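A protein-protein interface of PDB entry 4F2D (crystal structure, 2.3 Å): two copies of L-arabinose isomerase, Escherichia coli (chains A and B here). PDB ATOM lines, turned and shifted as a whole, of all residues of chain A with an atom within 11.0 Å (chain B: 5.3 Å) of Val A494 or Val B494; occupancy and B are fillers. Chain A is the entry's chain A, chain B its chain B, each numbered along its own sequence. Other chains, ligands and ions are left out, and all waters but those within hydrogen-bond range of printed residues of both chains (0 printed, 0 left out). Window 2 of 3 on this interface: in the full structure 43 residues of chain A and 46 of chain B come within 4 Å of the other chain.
Printed residues of chain B within 4 Å of Trp A491: Trp B491 (3.4 Å) and Asn B492 (2.8 Å).
Printed residues of chain B within 4 Å of Val A494: Val B494 and Tyr B495.
Of the printed residues of chain A, Trp B491 touches Trp A491 (3.4 Å).
Printed residues of chain A within 4 Å of Asn B492: Arg A490 (3.0 Å) and Trp A491 (2.8 Å).
Of chain A, only Val A494 (3.9 Å) comes within 4 Å of Val B494.
Printed residues of chain A within 4 Å of Tyr B496: Arg A490.
The nearest printed residue of chain B that does not touch Trp A491 is Tyr B495 (4.5 Å).
Printed residues of chain B that touch a printed residue of chain A: Trp B491, Asn B492, Val B494, Tyr B495 and Tyr B496.
Of the 18 printed residues of chain A, 3 touch a printed residue of chain B.
Hydrophobic or aromatic side chains of chain A that line the printed part of chain B: Trp A491 and Val A494.
Along chain A the printed residues that touch a printed residue of chain B span positions 490 to 494.
Among the printed residues, 7 pairs touch across the chains.
Among the printed residues, no Asp or Glu carboxylate lies within 4 Å of a Lys or Arg side-chain nitrogen of the other chain.
Arg A490 touches Asn B492, but with the chains exchanged Asn A492 does not touch Arg B490 (10.9 Å).
Arg A490 touches Tyr B495, but with the chains exchanged Tyr A495 does not touch Arg B490 (10.6 Å).
Val A494 touches its own counterpart, Val B494.
Val A494 touches Tyr B495, but with the chains exchanged Tyr A495 does not touch Val B494 (7.2 Å).
Of the 7 pairs that touch across the chains among the printed residues, 2 have their exchanged pair printed and touching as well.
Among the printed residues, pairs that only touch across the chains: Arg A490 with Tyr B495 (3.1 Å), Arg A490 with Tyr B496 (3.6 Å), Trp A491 with Trp B491 (3.4 Å), Val A494 with Val B494 (3.9 Å) and Val A494 with Tyr B495 (3.7 Å).
NH2 of Arg A490 lies within hydrogen-bond range of OD1 of Asn B492, 3.0 Å away.
OD1 of Asn B492 sits at hydrogen-bond distance from NE1 of Trp A491.
The side-chain carboxylate of Asp A487 lies within salt-bridge range of the guanidinium group of Arg A490, 2.8 Å away.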
ATOM      1  N   LEU A 399      22.329  17.666 -13.142  1.00  0.00           N
ATOM      2  CA  LEU A 399      20.877  17.531 -12.933  1.00  0.00           C
ATOM      3  C   LEU A 399      20.525  16.998 -11.540  1.00  0.00           C
ATOM      4  O   LEU A 399      19.355  16.746 -11.248  1.00  0.00           O
ATOM      5  CB  LEU A 399      20.252  16.635 -14.011  1.00  0.00           C
ATOM      6  CG  LEU A 399      20.157  17.231 -15.418  1.00  0.00           C
ATOM      7  CD1 LEU A 399      19.711  16.148 -16.392  1.00  0.00           C
ATOM      8  CD2 LEU A 399      19.204  18.417 -15.469  1.00  0.00           C
ATOM      9  N   ASP A 401      20.999  14.093 -10.037  1.00  0.00           N
ATOM     10  CA  ASP A 401      21.186  12.641 -10.068  1.00  0.00           C
ATOM     11  C   ASP A 401      22.092  12.179 -11.208  1.00  0.00           C
ATOM     12  O   ASP A 401      22.516  11.027 -11.234  1.00  0.00           O
ATOM     13  CB  ASP A 401      19.827  11.924 -10.151  1.00  0.00           C
ATOM     14  CG  ASP A 401      18.992  12.363 -11.349  1.00  0.00           C
ATOM     15  OD1 ASP A 401      19.277  13.427 -11.933  1.00  0.00           O
ATOM     16  OD2 ASP A 401      18.033  11.647 -11.698  1.00  0.00           O
ATOM     17  N   ARG A 402      22.383  13.073 -12.148  1.00  0.00           N
ATOM     18  CA  ARG A 402      23.216  12.745 -13.307  1.00  0.00           C
ATOM     19  C   ARG A 402      23.643  14.003 -14.059  1.00  0.00           C
ATOM     20  O   ARG A 402      23.152  15.103 -13.796  1.00  0.00           O
ATOM     21  CB  ARG A 402      22.473  11.798 -14.265  1.00  0.00           C
ATOM     22  CG  ARG A 402      21.163  12.355 -14.806  1.00  0.00           C
ATOM     23  CD  ARG A 402      20.431  11.350 -15.684  1.00  0.00           C
ATOM     24  NE  ARG A 402      19.238  11.944 -16.294  1.00  0.00           N
ATOM     25  CZ  ARG A 402      19.195  12.525 -17.490  1.00  0.00           C
ATOM     26  NH1 ARG A 402      20.277  12.602 -18.259  1.00  0.00           N
ATOM     27  NH2 ARG A 402      18.050  13.035 -17.928  1.00  0.00           N
ATOM     28  N   ARG A 404      24.274  16.125 -17.760  1.00  0.00           N
ATOM     29  CA  ARG A 404      23.820  16.317 -19.132  1.00  0.00           C
ATOM     30  C   ARG A 404      24.802  17.220 -19.861  1.00  0.00           C
ATOM     31  O   ARG A 404      25.156  18.286 -19.365  1.00  0.00           O
ATOM     32  CB  ARG A 404      22.422  16.943 -19.159  1.00  0.00           C
ATOM     33  CG  ARG A 404      21.872  17.200 -20.557  1.00  0.00           C
ATOM     34  CD  ARG A 404      20.520  17.901 -20.505  1.00  0.00           C
ATOM     35  NE  ARG A 404      19.425  16.979 -20.186  1.00  0.00           N
ATOM     36  CZ  ARG A 404      18.259  17.325 -19.639  1.00  0.00           C
ATOM     37  NH1 ARG A 404      17.997  18.588 -19.332  1.00  0.00           N
ATOM     38  NH2 ARG A 404      17.346  16.395 -19.390  1.00  0.00           N
ATOM     39  N   GLU A 472      24.177  11.667 -20.970  1.00  0.00           N
ATOM     40  CA  GLU A 472      23.277  12.148 -22.005  1.00  0.00           C
ATOM     41  C   GLU A 472      23.934  13.293 -22.765  1.00  0.00           C
ATOM     42  O   GLU A 472      24.474  14.217 -22.152  1.00  0.00           O
ATOM     43  CB  GLU A 472      21.956  12.631 -21.402  1.00  0.00           C
ATOM     44  CG  GLU A 472      20.972  13.184 -22.429  1.00  0.00           C
ATOM     45  CD  GLU A 472      19.714  13.748 -21.803  1.00  0.00           C
ATOM     46  OE1 GLU A 472      19.779  14.233 -20.651  1.00  0.00           O
ATOM     47  OE2 GLU A 472      18.658  13.714 -22.464  1.00  0.00           O
ATOM     48  N   LYS A 486      11.824  17.266 -27.416  1.00  0.00           N
ATOM     49  CA  LYS A 486      11.180  17.038 -26.118  1.00  0.00           C
ATOM     50  C   LYS A 486      10.958  15.557 -25.830  1.00  0.00           C
ATOM     51  O   LYS A 486      11.180  15.102 -24.707  1.00  0.00           O
ATOM     52  CB  LYS A 486       9.843  17.769 -26.030  1.00  0.00           C
ATOM     53  CG  LYS A 486       9.962  19.274 -25.896  1.00  0.00           C
ATOM     54  CD  LYS A 486       8.584  19.916 -25.939  1.00  0.00           C
ATOM     55  CE  LYS A 486       8.675  21.420 -26.093  1.00  0.00           C
ATOM     56  NZ  LYS A 486       7.334  22.033 -26.251  1.00  0.00           N
ATOM     57  N   ASP A 487      10.521  14.813 -26.843  1.00  0.00           N
ATOM     58  CA  ASP A 487      10.367  13.365 -26.721  1.00  0.00           C
ATOM     59  C   ASP A 487      11.669  12.735 -26.228  1.00  0.00           C
ATOM     60  O   ASP A 487      11.658  11.914 -25.319  1.00  0.00           O
ATOM     61  CB  ASP A 487       9.994  12.718 -28.064  1.00  0.00           C
ATOM     62  CG  ASP A 487       8.555  12.972 -28.488  1.00  0.00           C
ATOM     63  OD1 ASP A 487       8.226  12.774 -29.682  1.00  0.00           O
ATOM     64  OD2 ASP A 487       7.748  13.351 -27.632  1.00  0.00           O
ATOM     65  N   ALA A 488      12.780  13.121 -26.849  1.00  0.00           N
ATOM     66  CA  ALA A 488      14.097  12.577 -26.525  1.00  0.00           C
ATOM     67  C   ALA A 488      14.512  12.891 -25.086  1.00  0.00           C
ATOM     68  O   ALA A 488      15.063  12.036 -24.403  1.00  0.00           O
ATOM     69  CB  ALA A 488      15.142  13.102 -27.502  1.00  0.00           C
ATOM     70  N   LEU A 489      14.242  14.116 -24.640  1.00  0.00           N
ATOM     71  CA  LEU A 489      14.496  14.510 -23.246  1.00  0.00           C
ATOM     72  C   LEU A 489      13.780  13.585 -22.267  1.00  0.00           C
ATOM     73  O   LEU A 489      14.358  13.147 -21.272  1.00  0.00           O
ATOM     74  CB  LEU A 489      14.041  15.949 -22.984  1.00  0.00           C
ATOM     75  CG  LEU A 489      14.942  17.073 -23.489  1.00  0.00           C
ATOM     76  CD1 LEU A 489      14.304  18.409 -23.144  1.00  0.00           C
ATOM     77  CD2 LEU A 489      16.341  16.975 -22.886  1.00  0.00           C
ATOM     78  N   ARG A 490      12.521  13.285 -22.566  1.00  0.00           N
ATOM     79  CA  ARG A 490      11.724  12.399 -21.719  1.00  0.00           C
ATOM     80  C   ARG A 490      12.229  10.952 -21.753  1.00  0.00           C
ATOM     81  O   ARG A 490      12.401  10.324 -20.705  1.00  0.00           O
ATOM     82  CB  ARG A 490      10.256  12.458 -22.129  1.00  0.00           C
ATOM     83  CG  ARG A 490       9.610  13.806 -21.843  1.00  0.00           C
ATOM     84  CD  ARG A 490       8.115  13.824 -22.159  1.00  0.00           C
ATOM     85  NE  ARG A 490       7.742  12.833 -23.173  1.00  0.00           N
ATOM     86  CZ  ARG A 490       7.310  13.097 -24.411  1.00  0.00           C
ATOM     87  NH1 ARG A 490       7.171  14.352 -24.850  1.00  0.00           N
ATOM     88  NH2 ARG A 490       7.004  12.084 -25.227  1.00  0.00           N
ATOM     89  N   TRP A 491      12.482  10.434 -22.951  1.00  0.00           N
ATOM     90  CA  TRP A 491      12.908   9.041 -23.097  1.00  0.00           C
ATOM     91  C   TRP A 491      14.295   8.798 -22.560  1.00  0.00           C
ATOM     92  O   TRP A 491      14.581   7.720 -22.045  1.00  0.00           O
ATOM     93  CB  TRP A 491      12.804   8.577 -24.548  1.00  0.00           C
ATOM     94  CG  TRP A 491      11.405   8.672 -25.124  1.00  0.00           C
ATOM     95  CD1 TRP A 491      10.194   8.559 -24.446  1.00  0.00           C
ATOM     96  CD2 TRP A 491      11.030   8.875 -26.528  1.00  0.00           C
ATOM     97  NE1 TRP A 491       9.136   8.687 -25.305  1.00  0.00           N
ATOM     98  CE2 TRP A 491       9.567   8.882 -26.566  1.00  0.00           C
ATOM     99  CE3 TRP A 491      11.734   9.056 -27.708  1.00  0.00           C
ATOM    100  CZ2 TRP A 491       8.863   9.060 -27.749  1.00  0.00           C
ATOM    101  CZ3 TRP A 491      11.014   9.244 -28.894  1.00  0.00           C
ATOM    102  CH2 TRP A 491       9.613   9.240 -28.910  1.00  0.00           C
ATOM    103  N   ASN A 492      15.168   9.797 -22.672  1.00  0.00           N
ATOM    104  CA  ASN A 492      16.499   9.740 -22.049  1.00  0.00           C
ATOM    105  C   ASN A 492      16.419   9.816 -20.525  1.00  0.00           C
ATOM    106  O   ASN A 492      17.219   9.207 -19.826  1.00  0.00           O
ATOM    107  CB  ASN A 492      17.403  10.870 -22.559  1.00  0.00           C
ATOM    108  CG  ASN A 492      18.005  10.583 -23.924  1.00  0.00           C
ATOM    109  OD1 ASN A 492      17.939   9.467 -24.433  1.00  0.00           O
ATOM    110  ND2 ASN A 492      18.612  11.600 -24.516  1.00  0.00           N
ATOM    111  N   GLU A 493      15.460  10.584 -20.020  1.00  0.00           N
ATOM    112  CA  GLU A 493      15.290  10.754 -18.578  1.00  0.00           C
ATOM    113  C   GLU A 493      15.093   9.405 -17.887  1.00  0.00           C
ATOM    114  O   GLU A 493      15.727   9.128 -16.872  1.00  0.00           O
ATOM    115  CB  GLU A 493      14.113  11.685 -18.277  1.00  0.00           C
ATOM    116  CG  GLU A 493      13.807  11.853 -16.791  1.00  0.00           C
ATOM    117  CD  GLU A 493      14.641  12.933 -16.110  1.00  0.00           C
ATOM    118  OE1 GLU A 493      14.240  13.440 -15.041  1.00  0.00           O
ATOM    119  OE2 GLU A 493      15.708  13.282 -16.635  1.00  0.00           O
ATOM    120  N   VAL A 494      14.216   8.572 -18.439  1.00  0.00           N
ATOM    121  CA  VAL A 494      13.971   7.238 -17.869  1.00  0.00           C
ATOM    122  C   VAL A 494      15.128   6.268 -18.116  1.00  0.00           C
ATOM    123  O   VAL A 494      15.397   5.415 -17.278  1.00  0.00           O
ATOM    124  CB  VAL A 494      12.642   6.605 -18.340  1.00  0.00           C
ATOM    125  CG1 VAL A 494      11.472   7.251 -17.619  1.00  0.00           C
ATOM    126  CG2 VAL A 494      12.475   6.703 -19.847  1.00  0.00           C
ATOM    127  N   TYR A 495      15.824   6.403 -19.241  1.00  0.00           N
ATOM    128  CA  TYR A 495      16.991   5.554 -19.504  1.00  0.00           C
ATOM    129  C   TYR A 495      18.139   5.869 -18.546  1.00  0.00           C
ATOM    130  O   TYR A 495      18.611   4.987 -17.833  1.00  0.00           O
ATOM    131  CB  TYR A 495      17.490   5.683 -20.945  1.00  0.00           C
ATOM    132  CG  TYR A 495      18.765   4.893 -21.188  1.00  0.00           C
ATOM    133  CD1 TYR A 495      18.725   3.518 -21.381  1.00  0.00           C
ATOM    134  CD2 TYR A 495      20.012   5.516 -21.193  1.00  0.00           C
ATOM    135  CE1 TYR A 495      19.881   2.788 -21.588  1.00  0.00           C
ATOM    136  CE2 TYR A 495      21.175   4.793 -21.402  1.00  0.00           C
ATOM    137  CZ  TYR A 495      21.103   3.429 -21.597  1.00  0.00           C
ATOM    138  OH  TYR A 495      22.256   2.702 -21.801  1.00  0.00           O
ATOM    139  N   TYR A 496      18.594   7.121 -18.551  1.00  0.00           N
ATOM    140  CA  TYR A 496      19.734   7.532 -17.719  1.00  0.00           C
ATOM    141  C   TYR A 496      19.363   7.648 -16.242  1.00  0.00           C
ATOM    142  O   TYR A 496      20.238   7.665 -15.382  1.00  0.00           O
ATOM    143  CB  TYR A 496      20.339   8.848 -18.207  1.00  0.00           C
ATOM    144  CG  TYR A 496      21.039   8.731 -19.539  1.00  0.00           C
ATOM    145  CD1 TYR A 496      22.272   8.091 -19.645  1.00  0.00           C
ATOM    146  CD2 TYR A 496      20.468   9.251 -20.695  1.00  0.00           C
ATOM    147  CE1 TYR A 496      22.919   7.975 -20.866  1.00  0.00           C
ATOM    148  CE2 TYR A 496      21.104   9.141 -21.920  1.00  0.00           C
ATOM    149  CZ  TYR A 496      22.328   8.501 -22.003  1.00  0.00           C
ATOM    150  OH  TYR A 496      22.955   8.393 -23.228  1.00  0.00           O
ATOM    151  N   GLY A 497      18.069   7.717 -15.949  1.00  0.00           N
ATOM    152  CA  GLY A 497      17.591   7.666 -14.571  1.00  0.00           C
ATOM    153  C   GLY A 497      17.570   6.233 -14.073  1.00  0.00           C
ATOM    154  O   GLY A 497      16.537   5.723 -13.654  1.00  0.00           O
ATOM    155  N   PHE A 498      18.732   5.589 -14.145  1.00  0.00           N
ATOM    156  CA  PHE A 498      18.930   4.234 -13.641  1.00  0.00           C
ATOM    157  C   PHE A 498      20.236   4.139 -12.853  1.00  0.00           C
ATOM    158  O   PHE A 498      21.273   4.647 -13.289  1.00  0.00           O
ATOM    159  CB  PHE A 498      18.934   3.224 -14.803  1.00  0.00           C
ATOM    160  CG  PHE A 498      17.774   2.264 -14.791  1.00  0.00           C
ATOM    161  CD1 PHE A 498      16.487   2.729 -15.001  1.00  0.00           C
ATOM    162  CD2 PHE A 498      17.968   0.889 -14.595  1.00  0.00           C
ATOM    163  CE1 PHE A 498      15.407   1.864 -15.003  1.00  0.00           C
ATOM    164  CE2 PHE A 498      16.886   0.017 -14.597  1.00  0.00           C
ATOM    165  CZ  PHE A 498      15.605   0.506 -14.801  1.00  0.00           C
ATOM    166  N   ARG B 490       5.373   2.685 -27.020  1.00  0.00           N
ATOM    167  CA  ARG B 490       6.184   1.896 -26.093  1.00  0.00           C
ATOM    168  C   ARG B 490       7.083   2.777 -25.224  1.00  0.00           C
ATOM    169  O   ARG B 490       7.126   2.615 -24.004  1.00  0.00           O
ATOM    170  CB  ARG B 490       7.025   0.865 -26.851  1.00  0.00           C
ATOM    171  CG  ARG B 490       6.182  -0.236 -27.485  1.00  0.00           C
ATOM    172  CD  ARG B 490       6.987  -1.357 -28.118  1.00  0.00           C
ATOM    173  NE  ARG B 490       7.441  -1.044 -29.467  1.00  0.00           N
ATOM    174  CZ  ARG B 490       6.911  -1.538 -30.593  1.00  0.00           C
ATOM    175  NH1 ARG B 490       5.878  -2.391 -30.567  1.00  0.00           N
ATOM    176  NH2 ARG B 490       7.420  -1.173 -31.764  1.00  0.00           N
ATOM    177  N   TRP B 491       7.786   3.714 -25.852  1.00  0.00           N
ATOM    178  CA  TRP B 491       8.729   4.572 -25.128  1.00  0.00           C
ATOM    179  C   TRP B 491       8.033   5.522 -24.192  1.00  0.00           C
ATOM    180  O   TRP B 491       8.566   5.845 -23.138  1.00  0.00           O
ATOM    181  CB  TRP B 491       9.643   5.330 -26.085  1.00  0.00           C
ATOM    182  CG  TRP B 491      10.469   4.425 -26.972  1.00  0.00           C
ATOM    183  CD1 TRP B 491      10.936   3.150 -26.684  1.00  0.00           C
ATOM    184  CD2 TRP B 491      10.962   4.710 -28.327  1.00  0.00           C
ATOM    185  NE1 TRP B 491      11.652   2.644 -27.735  1.00  0.00           N
ATOM    186  CE2 TRP B 491      11.706   3.528 -28.748  1.00  0.00           C
ATOM    187  CE3 TRP B 491      10.865   5.785 -29.193  1.00  0.00           C
ATOM    188  CZ2 TRP B 491      12.312   3.449 -29.990  1.00  0.00           C
ATOM    189  CZ3 TRP B 491      11.483   5.696 -30.439  1.00  0.00           C
ATOM    190  CH2 TRP B 491      12.188   4.554 -30.827  1.00  0.00           C
ATOM    191  N   ASN B 492       6.843   5.979 -24.568  1.00  0.00           N
ATOM    192  CA  ASN B 492       6.015   6.799 -23.682  1.00  0.00           C
ATOM    193  C   ASN B 492       5.453   5.989 -22.519  1.00  0.00           C
ATOM    194  O   ASN B 492       5.302   6.502 -21.413  1.00  0.00           O
ATOM    195  CB  ASN B 492       4.856   7.441 -24.449  1.00  0.00           C
ATOM    196  CG  ASN B 492       5.276   8.662 -25.249  1.00  0.00           C
ATOM    197  OD1 ASN B 492       6.375   9.192 -25.084  1.00  0.00           O
ATOM    198  ND2 ASN B 492       4.390   9.124 -26.119  1.00  0.00           N
ATOM    199  N   GLU B 493       5.141   4.723 -22.772  1.00  0.00           N
ATOM    200  CA  GLU B 493       4.595   3.842 -21.743  1.00  0.00           C
ATOM    201  C   GLU B 493       5.522   3.767 -20.531  1.00  0.00           C
ATOM    202  O   GLU B 493       5.073   3.889 -19.393  1.00  0.00           O
ATOM    203  CB  GLU B 493       4.349   2.439 -22.309  1.00  0.00           C
ATOM    204  CG  GLU B 493       3.869   1.413 -21.295  1.00  0.00           C
ATOM    205  CD  GLU B 493       2.368   1.381 -21.128  1.00  0.00           C
ATOM    206  OE1 GLU B 493       1.711   2.426 -21.305  1.00  0.00           O
ATOM    207  OE2 GLU B 493       1.847   0.299 -20.802  1.00  0.00           O
ATOM    208  N   VAL B 494       6.811   3.562 -20.772  1.00  0.00           N
ATOM    209  CA  VAL B 494       7.779   3.489 -19.671  1.00  0.00           C
ATOM    210  C   VAL B 494       8.062   4.851 -19.043  1.00  0.00           C
ATOM    211  O   VAL B 494       8.314   4.930 -17.844  1.00  0.00           O
ATOM    212  CB  VAL B 494       9.105   2.826 -20.084  1.00  0.00           C
ATOM    213  CG1 VAL B 494       8.904   1.329 -20.247  1.00  0.00           C
ATOM    214  CG2 VAL B 494       9.650   3.445 -21.354  1.00  0.00           C
ATOM    215  N   TYR B 495       8.019   5.918 -19.841  1.00  0.00           N
ATOM    216  CA  TYR B 495       8.218   7.262 -19.297  1.00  0.00           C
ATOM    217  C   TYR B 495       7.073   7.668 -18.379  1.00  0.00           C
ATOM    218  O   TYR B 495       7.295   7.987 -17.216  1.00  0.00           O
ATOM    219  CB  TYR B 495       8.376   8.318 -20.391  1.00  0.00           C
ATOM    220  CG  TYR B 495       8.464   9.713 -19.814  1.00  0.00           C
ATOM    221  CD1 TYR B 495       9.641  10.174 -19.237  1.00  0.00           C
ATOM    222  CD2 TYR B 495       7.359  10.561 -19.814  1.00  0.00           C
ATOM    223  CE1 TYR B 495       9.725  11.446 -18.696  1.00  0.00           C
ATOM    224  CE2 TYR B 495       7.431  11.831 -19.276  1.00  0.00           C
ATOM    225  CZ  TYR B 495       8.616  12.268 -18.719  1.00  0.00           C
ATOM    226  OH  TYR B 495       8.691  13.525 -18.190  1.00  0.00           O
ATOM    227  N   TYR B 496       5.855   7.667 -18.917  1.00  0.00           N
ATOM    228  CA  TYR B 496       4.677   8.090 -18.154  1.00  0.00           C
ATOM    229  C   TYR B 496       4.252   7.057 -17.118  1.00  0.00           C
ATOM    230  O   TYR B 496       3.505   7.381 -16.201  1.00  0.00           O
ATOM    231  CB  TYR B 496       3.501   8.419 -19.080  1.00  0.00           C
ATOM    232  CG  TYR B 496       3.713   9.662 -19.904  1.00  0.00           C
ATOM    233  CD1 TYR B 496       3.653  10.925 -19.323  1.00  0.00           C
ATOM    234  CD2 TYR B 496       3.969   9.579 -21.270  1.00  0.00           C
ATOM    235  CE1 TYR B 496       3.849  12.072 -20.079  1.00  0.00           C
ATOM    236  CE2 TYR B 496       4.167  10.717 -22.031  1.00  0.00           C
ATOM    237  CZ  TYR B 496       4.107  11.960 -21.431  1.00  0.00           C
ATOM    238  OH  TYR B 496       4.316  13.090 -22.189  1.00  0.00           O
ATOM    239  N   GLY B 497       4.734   5.824 -17.267  1.00  0.00           N
ATOM    240  CA  GLY B 497       4.543   4.771 -16.269  1.00  0.00           C
ATOM    241  C   GLY B 497       5.680   4.719 -15.256  1.00  0.00           C
ATOM    242  O   GLY B 497       6.209   3.641 -14.957  1.00  0.00           O
ATOM    243  N   PHE B 498       6.033   5.882 -14.706  1.00  0.00           N
ATOM    244  CA  PHE B 498       7.318   6.061 -13.974  1.00  0.00           C
ATOM    245  C   PHE B 498       7.795   4.779 -13.311  1.00  0.00           C
ATOM    246  O   PHE B 498       8.628   4.076 -13.878  1.00  0.00           O
ATOM    247  CB  PHE B 498       7.301   7.223 -12.939  1.00  0.00           C
ATOM    248  CG  PHE B 498       5.941   7.543 -12.370  1.00  0.00           C
ATOM    249  CD1 PHE B 498       5.432   6.852 -11.271  1.00  0.00           C
ATOM    250  CD2 PHE B 498       5.182   8.572 -12.919  1.00  0.00           C
ATOM    251  CE1 PHE B 498       4.185   7.169 -10.750  1.00  0.00           C
ATOM    252  CE2 PHE B 498       3.933   8.890 -12.405  1.00  0.00           C
ATOM    253  CZ  PHE B 498       3.435   8.189 -11.317  1.00  0.00           C
